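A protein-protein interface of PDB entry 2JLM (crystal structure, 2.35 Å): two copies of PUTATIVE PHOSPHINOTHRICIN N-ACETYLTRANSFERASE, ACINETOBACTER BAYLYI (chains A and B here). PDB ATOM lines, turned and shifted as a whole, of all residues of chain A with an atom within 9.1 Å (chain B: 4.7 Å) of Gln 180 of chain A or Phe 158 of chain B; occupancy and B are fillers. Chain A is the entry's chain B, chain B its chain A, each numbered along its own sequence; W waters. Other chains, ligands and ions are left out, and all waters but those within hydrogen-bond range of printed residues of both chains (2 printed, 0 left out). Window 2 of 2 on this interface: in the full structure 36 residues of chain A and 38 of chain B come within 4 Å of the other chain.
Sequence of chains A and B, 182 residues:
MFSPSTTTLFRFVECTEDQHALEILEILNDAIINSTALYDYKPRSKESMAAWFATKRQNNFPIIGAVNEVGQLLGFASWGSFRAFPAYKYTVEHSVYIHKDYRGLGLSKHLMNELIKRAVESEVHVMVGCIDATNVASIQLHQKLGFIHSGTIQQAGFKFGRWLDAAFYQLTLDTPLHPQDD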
ATOM      1  N   PHE A  85     -12.859 -30.810  17.594  1.00  0.00           N
ATOM      2  CA  PHE A  85     -11.978 -30.047  16.734  1.00  0.00           C
ATOM      3  C   PHE A  85     -10.960 -29.431  17.659  1.00  0.00           C
ATOM      4  O   PHE A  85     -11.296 -29.076  18.787  1.00  0.00           O
ATOM      5  CB  PHE A  85     -12.733 -28.941  15.997  1.00  0.00           C
ATOM      6  CG  PHE A  85     -13.714 -29.449  14.996  1.00  0.00           C
ATOM      7  CD1 PHE A  85     -14.919 -29.995  15.407  1.00  0.00           C
ATOM      8  CD2 PHE A  85     -13.436 -29.380  13.640  1.00  0.00           C
ATOM      9  CE1 PHE A  85     -15.830 -30.470  14.483  1.00  0.00           C
ATOM     10  CE2 PHE A  85     -14.345 -29.849  12.709  1.00  0.00           C
ATOM     11  CZ  PHE A  85     -15.543 -30.395  13.131  1.00  0.00           C
ATOM     12  N   PRO A  86      -9.708 -29.319  17.191  1.00  0.00           N
ATOM     13  CA  PRO A  86      -8.598 -28.905  18.053  1.00  0.00           C
ATOM     14  C   PRO A  86      -8.832 -27.603  18.814  1.00  0.00           C
ATOM     15  O   PRO A  86      -8.426 -27.517  19.968  1.00  0.00           O
ATOM     16  CB  PRO A  86      -7.427 -28.760  17.065  1.00  0.00           C
ATOM     17  CG  PRO A  86      -7.718 -29.766  16.020  1.00  0.00           C
ATOM     18  CD  PRO A  86      -9.237 -29.766  15.864  1.00  0.00           C
ATOM     19  N   ALA A  87      -9.465 -26.611  18.199  1.00  0.00           N
ATOM     20  CA  ALA A  87      -9.612 -25.302  18.863  1.00  0.00           C
ATOM     21  C   ALA A  87     -10.647 -25.299  19.998  1.00  0.00           C
ATOM     22  O   ALA A  87     -10.851 -24.277  20.660  1.00  0.00           O
ATOM     23  CB  ALA A  87      -9.910 -24.203  17.840  1.00  0.00           C
ATOM     24  N   TYR A  88     -11.291 -26.445  20.216  1.00  0.00           N
ATOM     25  CA  TYR A  88     -12.183 -26.643  21.361  1.00  0.00           C
ATOM     26  C   TYR A  88     -11.445 -27.258  22.556  1.00  0.00           C
ATOM     27  O   TYR A  88     -12.066 -27.707  23.522  1.00  0.00           O
ATOM     28  CB  TYR A  88     -13.350 -27.556  20.979  1.00  0.00           C
ATOM     29  CG  TYR A  88     -14.397 -26.901  20.122  1.00  0.00           C
ATOM     30  CD1 TYR A  88     -14.459 -27.154  18.751  1.00  0.00           C
ATOM     31  CD2 TYR A  88     -15.335 -26.037  20.678  1.00  0.00           C
ATOM     32  CE1 TYR A  88     -15.415 -26.553  17.958  1.00  0.00           C
ATOM     33  CE2 TYR A  88     -16.302 -25.430  19.890  1.00  0.00           C
ATOM     34  CZ  TYR A  88     -16.339 -25.696  18.538  1.00  0.00           C
ATOM     35  OH  TYR A  88     -17.302 -25.110  17.763  1.00  0.00           O
ATOM     36  N   LYS A  89     -10.119 -27.264  22.488  1.00  0.00           N
ATOM     37  CA  LYS A  89      -9.277 -27.908  23.496  1.00  0.00           C
ATOM     38  C   LYS A  89      -9.580 -27.506  24.944  1.00  0.00           C
ATOM     39  O   LYS A  89      -9.371 -28.297  25.866  1.00  0.00           O
ATOM     40  CB  LYS A  89      -7.800 -27.638  23.193  1.00  0.00           C
ATOM     41  CG  LYS A  89      -7.429 -26.174  23.235  1.00  0.00           C
ATOM     42  CD  LYS A  89      -6.169 -25.897  22.431  1.00  0.00           C
ATOM     43  CE  LYS A  89      -4.923 -26.054  23.272  1.00  0.00           C
ATOM     44  NZ  LYS A  89      -3.781 -25.366  22.612  1.00  0.00           N
ATOM     45  N   TYR A  90     -10.063 -26.287  25.146  1.00  0.00           N
ATOM     46  CA  TYR A  90     -10.327 -25.798  26.496  1.00  0.00           C
ATOM     47  C   TYR A  90     -11.805 -25.920  26.882  1.00  0.00           C
ATOM     48  O   TYR A  90     -12.230 -25.358  27.887  1.00  0.00           O
ATOM     49  CB  TYR A  90      -9.859 -24.343  26.656  1.00  0.00           C
ATOM     50  CG  TYR A  90      -8.375 -24.116  26.416  1.00  0.00           C
ATOM     51  CD1 TYR A  90      -7.416 -24.676  27.254  1.00  0.00           C
ATOM     52  CD2 TYR A  90      -7.934 -23.319  25.367  1.00  0.00           C
ATOM     53  CE1 TYR A  90      -6.056 -24.460  27.044  1.00  0.00           C
ATOM     54  CE2 TYR A  90      -6.577 -23.093  25.147  1.00  0.00           C
ATOM     55  CZ  TYR A  90      -5.643 -23.666  25.991  1.00  0.00           C
ATOM     56  OH  TYR A  90      -4.297 -23.443  25.785  1.00  0.00           O
ATOM     57  N   THR A  91     -12.582 -26.658  26.092  1.00  0.00           N
ATOM     58  CA  THR A  91     -14.003 -26.832  26.387  1.00  0.00           C
ATOM     59  C   THR A  91     -14.345 -28.290  26.663  1.00  0.00           C
ATOM     60  O   THR A  91     -13.940 -29.190  25.924  1.00  0.00           O
ATOM     61  CB  THR A  91     -14.892 -26.336  25.227  1.00  0.00           C
ATOM     62  OG1 THR A  91     -14.650 -24.943  24.989  1.00  0.00           O
ATOM     63  CG2 THR A  91     -16.353 -26.534  25.555  1.00  0.00           C
ATOM     64  N   GLU A 123      -7.225 -26.920  33.910  1.00  0.00           N
ATOM     65  CA  GLU A 123      -7.066 -25.872  32.901  1.00  0.00           C
ATOM     66  C   GLU A 123      -8.237 -25.803  31.918  1.00  0.00           C
ATOM     67  O   GLU A 123      -8.078 -25.366  30.780  1.00  0.00           O
ATOM     68  CB  GLU A 123      -5.745 -26.042  32.143  1.00  0.00           C
ATOM     69  CG  GLU A 123      -4.506 -25.790  32.988  1.00  0.00           C
ATOM     70  CD  GLU A 123      -4.232 -24.312  33.210  1.00  0.00           C
ATOM     71  OE1 GLU A 123      -4.523 -23.814  34.318  1.00  0.00           O
ATOM     72  OE2 GLU A 123      -3.728 -23.650  32.277  1.00  0.00           O
ATOM     73  N   HIS A 125     -11.462 -24.141  30.414  1.00  0.00           N
ATOM     74  CA  HIS A 125     -11.991 -22.779  30.340  1.00  0.00           C
ATOM     75  C   HIS A 125     -13.527 -22.737  30.379  1.00  0.00           C
ATOM     76  O   HIS A 125     -14.115 -21.877  31.026  1.00  0.00           O
ATOM     77  CB  HIS A 125     -11.471 -22.069  29.086  1.00  0.00           C
ATOM     78  CG  HIS A 125     -11.921 -20.647  28.966  1.00  0.00           C
ATOM     79  ND1 HIS A 125     -11.737 -19.721  29.971  1.00  0.00           N
ATOM     80  CD2 HIS A 125     -12.532 -19.987  27.954  1.00  0.00           C
ATOM     81  CE1 HIS A 125     -12.228 -18.555  29.587  1.00  0.00           C
ATOM     82  NE2 HIS A 125     -12.705 -18.685  28.363  1.00  0.00           N
ATOM     83  N   VAL A 126     -14.173 -23.669  29.689  1.00  0.00           N
ATOM     84  CA  VAL A 126     -15.635 -23.699  29.628  1.00  0.00           C
ATOM     85  C   VAL A 126     -16.161 -25.114  29.874  1.00  0.00           C
ATOM     86  O   VAL A 126     -15.723 -26.082  29.235  1.00  0.00           O
ATOM     87  CB  VAL A 126     -16.157 -23.215  28.243  1.00  0.00           C
ATOM     88  CG1 VAL A 126     -17.656 -23.344  28.166  1.00  0.00           C
ATOM     89  CG2 VAL A 126     -15.746 -21.779  27.963  1.00  0.00           C
ATOM     90  N   PRO A 176      -7.792 -21.382  31.364  1.00  0.00           N
ATOM     91  CA  PRO A 176      -6.371 -21.385  31.720  1.00  0.00           C
ATOM     92  C   PRO A 176      -5.845 -19.963  31.686  1.00  0.00           C
ATOM     93  O   PRO A 176      -6.388 -19.131  30.952  1.00  0.00           O
ATOM     94  CB  PRO A 176      -5.741 -22.180  30.585  1.00  0.00           C
ATOM     95  CG  PRO A 176      -6.614 -21.876  29.402  1.00  0.00           C
ATOM     96  CD  PRO A 176      -8.001 -21.613  29.925  1.00  0.00           C
ATOM     97  N   LEU A 177      -4.798 -19.697  32.460  1.00  0.00           N
ATOM     98  CA  LEU A 177      -4.209 -18.363  32.531  1.00  0.00           C
ATOM     99  C   LEU A 177      -3.510 -17.938  31.244  1.00  0.00           C
ATOM    100  O   LEU A 177      -3.539 -16.757  30.882  1.00  0.00           O
ATOM    101  CB  LEU A 177      -3.233 -18.281  33.702  1.00  0.00           C
ATOM    102  CG  LEU A 177      -3.797 -17.626  34.955  1.00  0.00           C
ATOM    103  CD1 LEU A 177      -3.021 -18.057  36.188  1.00  0.00           C
ATOM    104  CD2 LEU A 177      -3.759 -16.118  34.780  1.00  0.00           C
ATOM    105  N   HIS A 178      -2.876 -18.894  30.563  1.00  0.00           N
ATOM    106  CA  HIS A 178      -2.148 -18.596  29.327  1.00  0.00           C
ATOM    107  C   HIS A 178      -2.549 -19.527  28.181  1.00  0.00           C
ATOM    108  O   HIS A 178      -1.809 -20.448  27.832  1.00  0.00           O
ATOM    109  CB  HIS A 178      -0.632 -18.650  29.563  1.00  0.00           C
ATOM    110  CG  HIS A 178      -0.174 -17.793  30.704  1.00  0.00           C
ATOM    111  ND1 HIS A 178       0.014 -16.432  30.579  1.00  0.00           N
ATOM    112  CD2 HIS A 178       0.116 -18.099  31.989  1.00  0.00           C
ATOM    113  CE1 HIS A 178       0.401 -15.938  31.741  1.00  0.00           C
ATOM    114  NE2 HIS A 178       0.472 -16.927  32.616  1.00  0.00           N
ATOM    115  N   PRO A 179      -3.731 -19.286  27.592  1.00  0.00           N
ATOM    116  CA  PRO A 179      -4.254 -20.110  26.497  1.00  0.00           C
ATOM    117  C   PRO A 179      -3.399 -19.935  25.253  1.00  0.00           C
ATOM    118  O   PRO A 179      -2.951 -18.813  24.998  1.00  0.00           O
ATOM    119  CB  PRO A 179      -5.629 -19.489  26.243  1.00  0.00           C
ATOM    120  CG  PRO A 179      -5.461 -18.043  26.704  1.00  0.00           C
ATOM    121  CD  PRO A 179      -4.682 -18.221  27.963  1.00  0.00           C
ATOM    122  N   GLN A 180      -3.186 -21.002  24.484  1.00  0.00           N
ATOM    123  CA  GLN A 180      -2.444 -20.869  23.224  1.00  0.00           C
ATOM    124  C   GLN A 180      -2.944 -21.792  22.110  1.00  0.00           C
ATOM    125  O   GLN A 180      -3.450 -22.883  22.384  1.00  0.00           O
ATOM    126  CB  GLN A 180      -0.931 -21.064  23.457  1.00  0.00           C
ATOM    127  CG  GLN A 180      -0.550 -22.278  24.298  1.00  0.00           C
ATOM    128  N   ASP A 181      -2.806 -21.348  20.857  1.00  0.00           N
ATOM    129  CA  ASP A 181      -3.088 -22.205  19.700  1.00  0.00           C
ATOM    130  C   ASP A 181      -2.221 -23.445  19.818  1.00  0.00           C
ATOM    131  O   ASP A 181      -1.146 -23.383  20.411  1.00  0.00           O
ATOM    132  CB  ASP A 181      -2.760 -21.490  18.379  1.00  0.00           C
ATOM    133  CG  ASP A 181      -3.770 -20.400  18.018  1.00  0.00           C
ATOM    134  OD1 ASP A 181      -4.090 -20.257  16.814  1.00  0.00           O
ATOM    135  OD2 ASP A 181      -4.237 -19.680  18.929  1.00  0.00           O
ATOM    136  N   ASP A 182      -2.670 -24.570  19.264  1.00  0.00           N
ATOM    137  CA  ASP A 182      -1.836 -25.774  19.252  1.00  0.00           C
ATOM    138  C   ASP A 182      -0.517 -25.516  18.524  1.00  0.00           C
ATOM    139  O   ASP A 182       0.543 -26.011  18.916  1.00  0.00           O
ATOM    140  CB  ASP A 182      -2.558 -26.942  18.583  1.00  0.00           C
ATOM    141  CG  ASP A 182      -3.406 -27.735  19.552  1.00  0.00           C
ATOM    142  OD1 ASP A 182      -4.065 -28.697  19.093  1.00  0.00           O
ATOM    143  OD2 ASP A 182      -3.416 -27.403  20.763  1.00  0.00           O
ATOM    144  OXT ASP A 182      -0.486 -24.801  17.521  1.00  0.00           O
ATOM    145  N   TYR B  41      -6.209 -26.159  13.665  1.00  0.00           N
ATOM    146  CA  TYR B  41      -5.060 -25.253  13.659  1.00  0.00           C
ATOM    147  C   TYR B  41      -4.168 -25.538  12.447  1.00  0.00           C
ATOM    148  O   TYR B  41      -3.761 -24.627  11.732  1.00  0.00           O
ATOM    149  CB  TYR B  41      -4.236 -25.411  14.932  1.00  0.00           C
ATOM    150  CG  TYR B  41      -4.940 -25.023  16.213  1.00  0.00           C
ATOM    151  CD1 TYR B  41      -5.341 -25.988  17.133  1.00  0.00           C
ATOM    152  CD2 TYR B  41      -5.187 -23.692  16.514  1.00  0.00           C
ATOM    153  CE1 TYR B  41      -5.977 -25.631  18.322  1.00  0.00           C
ATOM    154  CE2 TYR B  41      -5.824 -23.325  17.697  1.00  0.00           C
ATOM    155  CZ  TYR B  41      -6.214 -24.293  18.595  1.00  0.00           C
ATOM    156  OH  TYR B  41      -6.841 -23.921  19.765  1.00  0.00           O
ATOM    157  N   ALA B 156     -15.923 -20.694  23.399  1.00  0.00           N
ATOM    158  CA  ALA B 156     -15.826 -22.141  23.249  1.00  0.00           C
ATOM    159  C   ALA B 156     -14.533 -22.527  22.548  1.00  0.00           C
ATOM    160  O   ALA B 156     -14.005 -23.625  22.746  1.00  0.00           O
ATOM    161  CB  ALA B 156     -17.000 -22.660  22.481  1.00  0.00           C
ATOM    162  N   GLY B 157     -14.031 -21.620  21.716  1.00  0.00           N
ATOM    163  CA  GLY B 157     -12.843 -21.893  20.940  1.00  0.00           C
ATOM    164  C   GLY B 157     -11.682 -20.961  21.215  1.00  0.00           C
ATOM    165  O   GLY B 157     -11.839 -19.862  21.744  1.00  0.00           O
ATOM    166  N   PHE B 158     -10.496 -21.412  20.848  1.00  0.00           N
ATOM    167  CA  PHE B 158      -9.330 -20.565  20.927  1.00  0.00           C
ATOM    168  C   PHE B 158      -8.512 -20.727  19.658  1.00  0.00           C
ATOM    169  O   PHE B 158      -8.078 -21.830  19.338  1.00  0.00           O
ATOM    170  CB  PHE B 158      -8.492 -20.910  22.165  1.00  0.00           C
ATOM    171  CG  PHE B 158      -7.447 -19.885  22.472  1.00  0.00           C
ATOM    172  CD1 PHE B 158      -7.742 -18.798  23.278  1.00  0.00           C
ATOM    173  CD2 PHE B 158      -6.181 -19.981  21.916  1.00  0.00           C
ATOM    174  CE1 PHE B 158      -6.782 -17.838  23.544  1.00  0.00           C
ATOM    175  CE2 PHE B 158      -5.216 -19.021  22.180  1.00  0.00           C
ATOM    176  CZ  PHE B 158      -5.520 -17.948  22.993  1.00  0.00           C
ATOM    177  N   LYS B 159      -8.316 -19.630  18.933  1.00  0.00           N
ATOM    178  CA  LYS B 159      -7.551 -19.648  17.693  1.00  0.00           C
ATOM    179  C   LYS B 159      -7.059 -18.239  17.355  1.00  0.00           C
ATOM    180  O   LYS B 159      -7.695 -17.258  17.719  1.00  0.00           O
ATOM    181  CB  LYS B 159      -8.386 -20.224  16.540  1.00  0.00           C
ATOM    182  CG  LYS B 159      -7.551 -20.690  15.344  1.00  0.00           C
ATOM    183  CD  LYS B 159      -8.397 -21.246  14.213  1.00  0.00           C
ATOM    184  CE  LYS B 159      -7.594 -21.317  12.921  1.00  0.00           C
ATOM    185  NZ  LYS B 159      -8.283 -22.125  11.885  1.00  0.00           N
ATOM    186  N   GLY B 161      -4.703 -16.739  18.705  1.00  0.00           N
ATOM    187  CA  GLY B 161      -4.465 -16.085  19.976  1.00  0.00           C
ATOM    188  C   GLY B 161      -5.670 -15.401  20.595  1.00  0.00           C
ATOM    189  O   GLY B 161      -5.518 -14.450  21.362  1.00  0.00           O
ATOM    190  N   ARG B 162      -6.870 -15.879  20.288  1.00  0.00           N
ATOM    191  CA  ARG B 162      -8.073 -15.317  20.907  1.00  0.00           C
ATOM    192  C   ARG B 162      -9.212 -16.311  21.146  1.00  0.00           C
ATOM    193  O   ARG B 162      -9.291 -17.382  20.522  1.00  0.00           O
ATOM    194  CB  ARG B 162      -8.592 -14.142  20.087  1.00  0.00           C
ATOM    195  CG  ARG B 162      -9.115 -14.536  18.733  1.00  0.00           C
ATOM    196  CD  ARG B 162      -9.710 -13.342  18.032  1.00  0.00           C
ATOM    197  NE  ARG B 162     -10.956 -13.708  17.376  1.00  0.00           N
ATOM    198  CZ  ARG B 162     -11.075 -13.954  16.079  1.00  0.00           C
ATOM    199  NH1 ARG B 162     -12.260 -14.289  15.571  1.00  0.00           N
ATOM    200  NH2 ARG B 162     -10.012 -13.856  15.294  1.00  0.00           N
ATOM    201  N   TRP B 163     -10.093 -15.929  22.061  1.00  0.00           N
ATOM    202  CA  TRP B 163     -11.291 -16.699  22.374  1.00  0.00           C
ATOM    203  C   TRP B 163     -12.332 -16.559  21.268  1.00  0.00           C
ATOM    204  O   TRP B 163     -12.570 -15.462  20.764  1.00  0.00           O
ATOM    205  CB  TRP B 163     -11.893 -16.235  23.705  1.00  0.00           C
ATOM    206  CG  TRP B 163     -11.044 -16.571  24.880  1.00  0.00           C
ATOM    207  CD1 TRP B 163     -10.466 -15.696  25.755  1.00  0.00           C
ATOM    208  CD2 TRP B 163     -10.668 -17.881  25.314  1.00  0.00           C
ATOM    209  NE1 TRP B 163      -9.763 -16.382  26.714  1.00  0.00           N
ATOM    210  CE2 TRP B 163      -9.866 -17.725  26.465  1.00  0.00           C
ATOM    211  CE3 TRP B 163     -10.934 -19.168  24.848  1.00  0.00           C
ATOM    212  CZ2 TRP B 163      -9.318 -18.807  27.144  1.00  0.00           C
ATOM    213  CZ3 TRP B 163     -10.392 -20.241  25.523  1.00  0.00           C
ATOM    214  CH2 TRP B 163      -9.590 -20.055  26.660  1.00  0.00           C
ATOM    215  N   LEU B 164     -12.954 -17.676  20.896  1.00  0.00           N
ATOM    216  CA  LEU B 164     -13.979 -17.669  19.851  1.00  0.00           C
ATOM    217  C   LEU B 164     -15.365 -18.007  20.394  1.00  0.00           C
ATOM    218  O   LEU B 164     -15.520 -18.891  21.236  1.00  0.00           O
ATOM    219  CB  LEU B 164     -13.633 -18.668  18.757  1.00  0.00           C
ATOM    220  CG  LEU B 164     -12.269 -18.568  18.077  1.00  0.00           C
ATOM    221  CD1 LEU B 164     -12.177 -19.665  17.060  1.00  0.00           C
ATOM    222  CD2 LEU B 164     -12.081 -17.227  17.393  1.00  0.00           C
HETATM  223  O   HOH W   1     -12.625 -22.830  25.608  1.00  0.00           O
HETATM  224  O   HOH W   2     -11.057 -24.072  23.717  1.00  0.00           O
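O of Ala 156 of chain B sits at hydrogen-bond distance from OG1 of Thr 91 of chain A (2.7 Å). N of Phe 158 of chain B sits at hydrogen-bond distance from O of Ala 87 of chain A, at 2.9 Å. N of Gly 161 of chain B is in hydrogen-bond range of OD2 of Asp 181 of chain A, at 3.0 Å.
N of Leu 164 of chain B sits at hydrogen-bond distance from O of Gly 157 of chain B (2.6 Å). The side-chain amino group of Lys 89 of chain A lies within hydrogen-bond range of the backbone carbonyl oxygen of Gln 180 of chain A (2.5 Å). OD2 of Asp 182 of chain A lies within salt-bridge range of NZ of Lys 89 of chain A (2.8 Å). O of Tyr 90 of chain A lies within hydrogen-bond range of N of His 125 of chain A, 2.9 Å away. N of Val 126 of chain A lies within hydrogen-bond range of O of Tyr 90 of chain A, 3.1 Å away. OH of Tyr 90 of chain A sits at hydrogen-bond distance from N of Gln 180 of chain A.
Tyr 41 of chain B touches Pro 86 of chain A (CD1 to CB, 3.5 Å). Ala 87 of chain A touches Ala 156 of chain B. CA of Gly 157 of chain B touches O of Ala 87 of chain A (3.1 Å). Ala 156 of chain B touches Tyr 88 of chain A (O to CD2, 3.4 Å). Trp 163 of chain B touches His 125 of chain A (CH2 to CD2, 3.2 Å). Pro 176 of chain A touches Trp 163 of chain B (CD to CH2, 3.95 Å). Phe 158 of chain B touches Pro 179 of chain A (CE1 to CB, 3.4 Å). Trp 163 of chain B touches Pro 179 of chain A (CZ2 to CB, 3.9 Å). CA of Gln 180 of chain A touches CE2 of Phe 158 of chain B, 3.5 Å away. OD2 of Asp 181 of chain A touches CE2 of Phe 158 of chain B, at 3.5 Å.
Printed residues of chain B within 4 Å of Gln 180 of chain A: Phe 158 (3.5 Å). Of chain A, only Ala 87, Pro 179, Gln 180 and Asp 181 come within 4 Å of Phe 158 of chain B. Of chain A, only Ala 87 comes within 4 Å of Gly 157 of chain B. Of chain A, only Asp 181 comes within 4 Å of Gly 161 of chain B. Printed residues of chain B within 4 Å of His 125 of chain A: Trp 163 (3.2 Å). Of the printed residues of chain A, Tyr 41 of chain B touches Pro 86, Ala 87, Lys 89, Asp 181 and Asp 182. The nearest residue of chain A that does not touch Phe 158 of chain B is Tyr 90 of chain A (4.05 Å). The nearest printed residue of chain B that does not touch Thr 91 of chain A is Gly 157 of chain B (4.7 Å).
Printed residues of chain A that touch a printed residue of chain B: Pro 86, Ala 87, Tyr 88, Lys 89, Tyr 90, Thr 91, His 125, Pro 176, Pro 179, Gln 180, Asp 181 and Asp 182. Along chain A the printed residues that touch a printed residue of chain B span positions 86 to 182. Of the 9 printed residues of chain B, 7 touch a printed residue of chain A. Hydrophobic or aromatic side chains of chain B that line the printed part of chain A: Tyr 41, Ala 156, Phe 158 and Trp 163.
No position is printed for both chains.
Water W2 lies within hydrogen-bond range of the backbone NH of Tyr 90 of chain A (2.8 Å), the backbone carbonyl oxygen of Ala 87 of chain A (3.1 Å) and the backbone carbonyl oxygen of Ala 156 of chain B (3.1 Å). Water W1 lies within hydrogen-bond range of the side-chain hydroxyl (OG1) of Thr 91 of chain A (3.0 Å), the backbone carbonyl oxygen (O) of Ala 156 of chain B (3.3 Å) and the backbone carbonyl oxygen (O) of Tyr 90 of chain A (3.4 Å).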
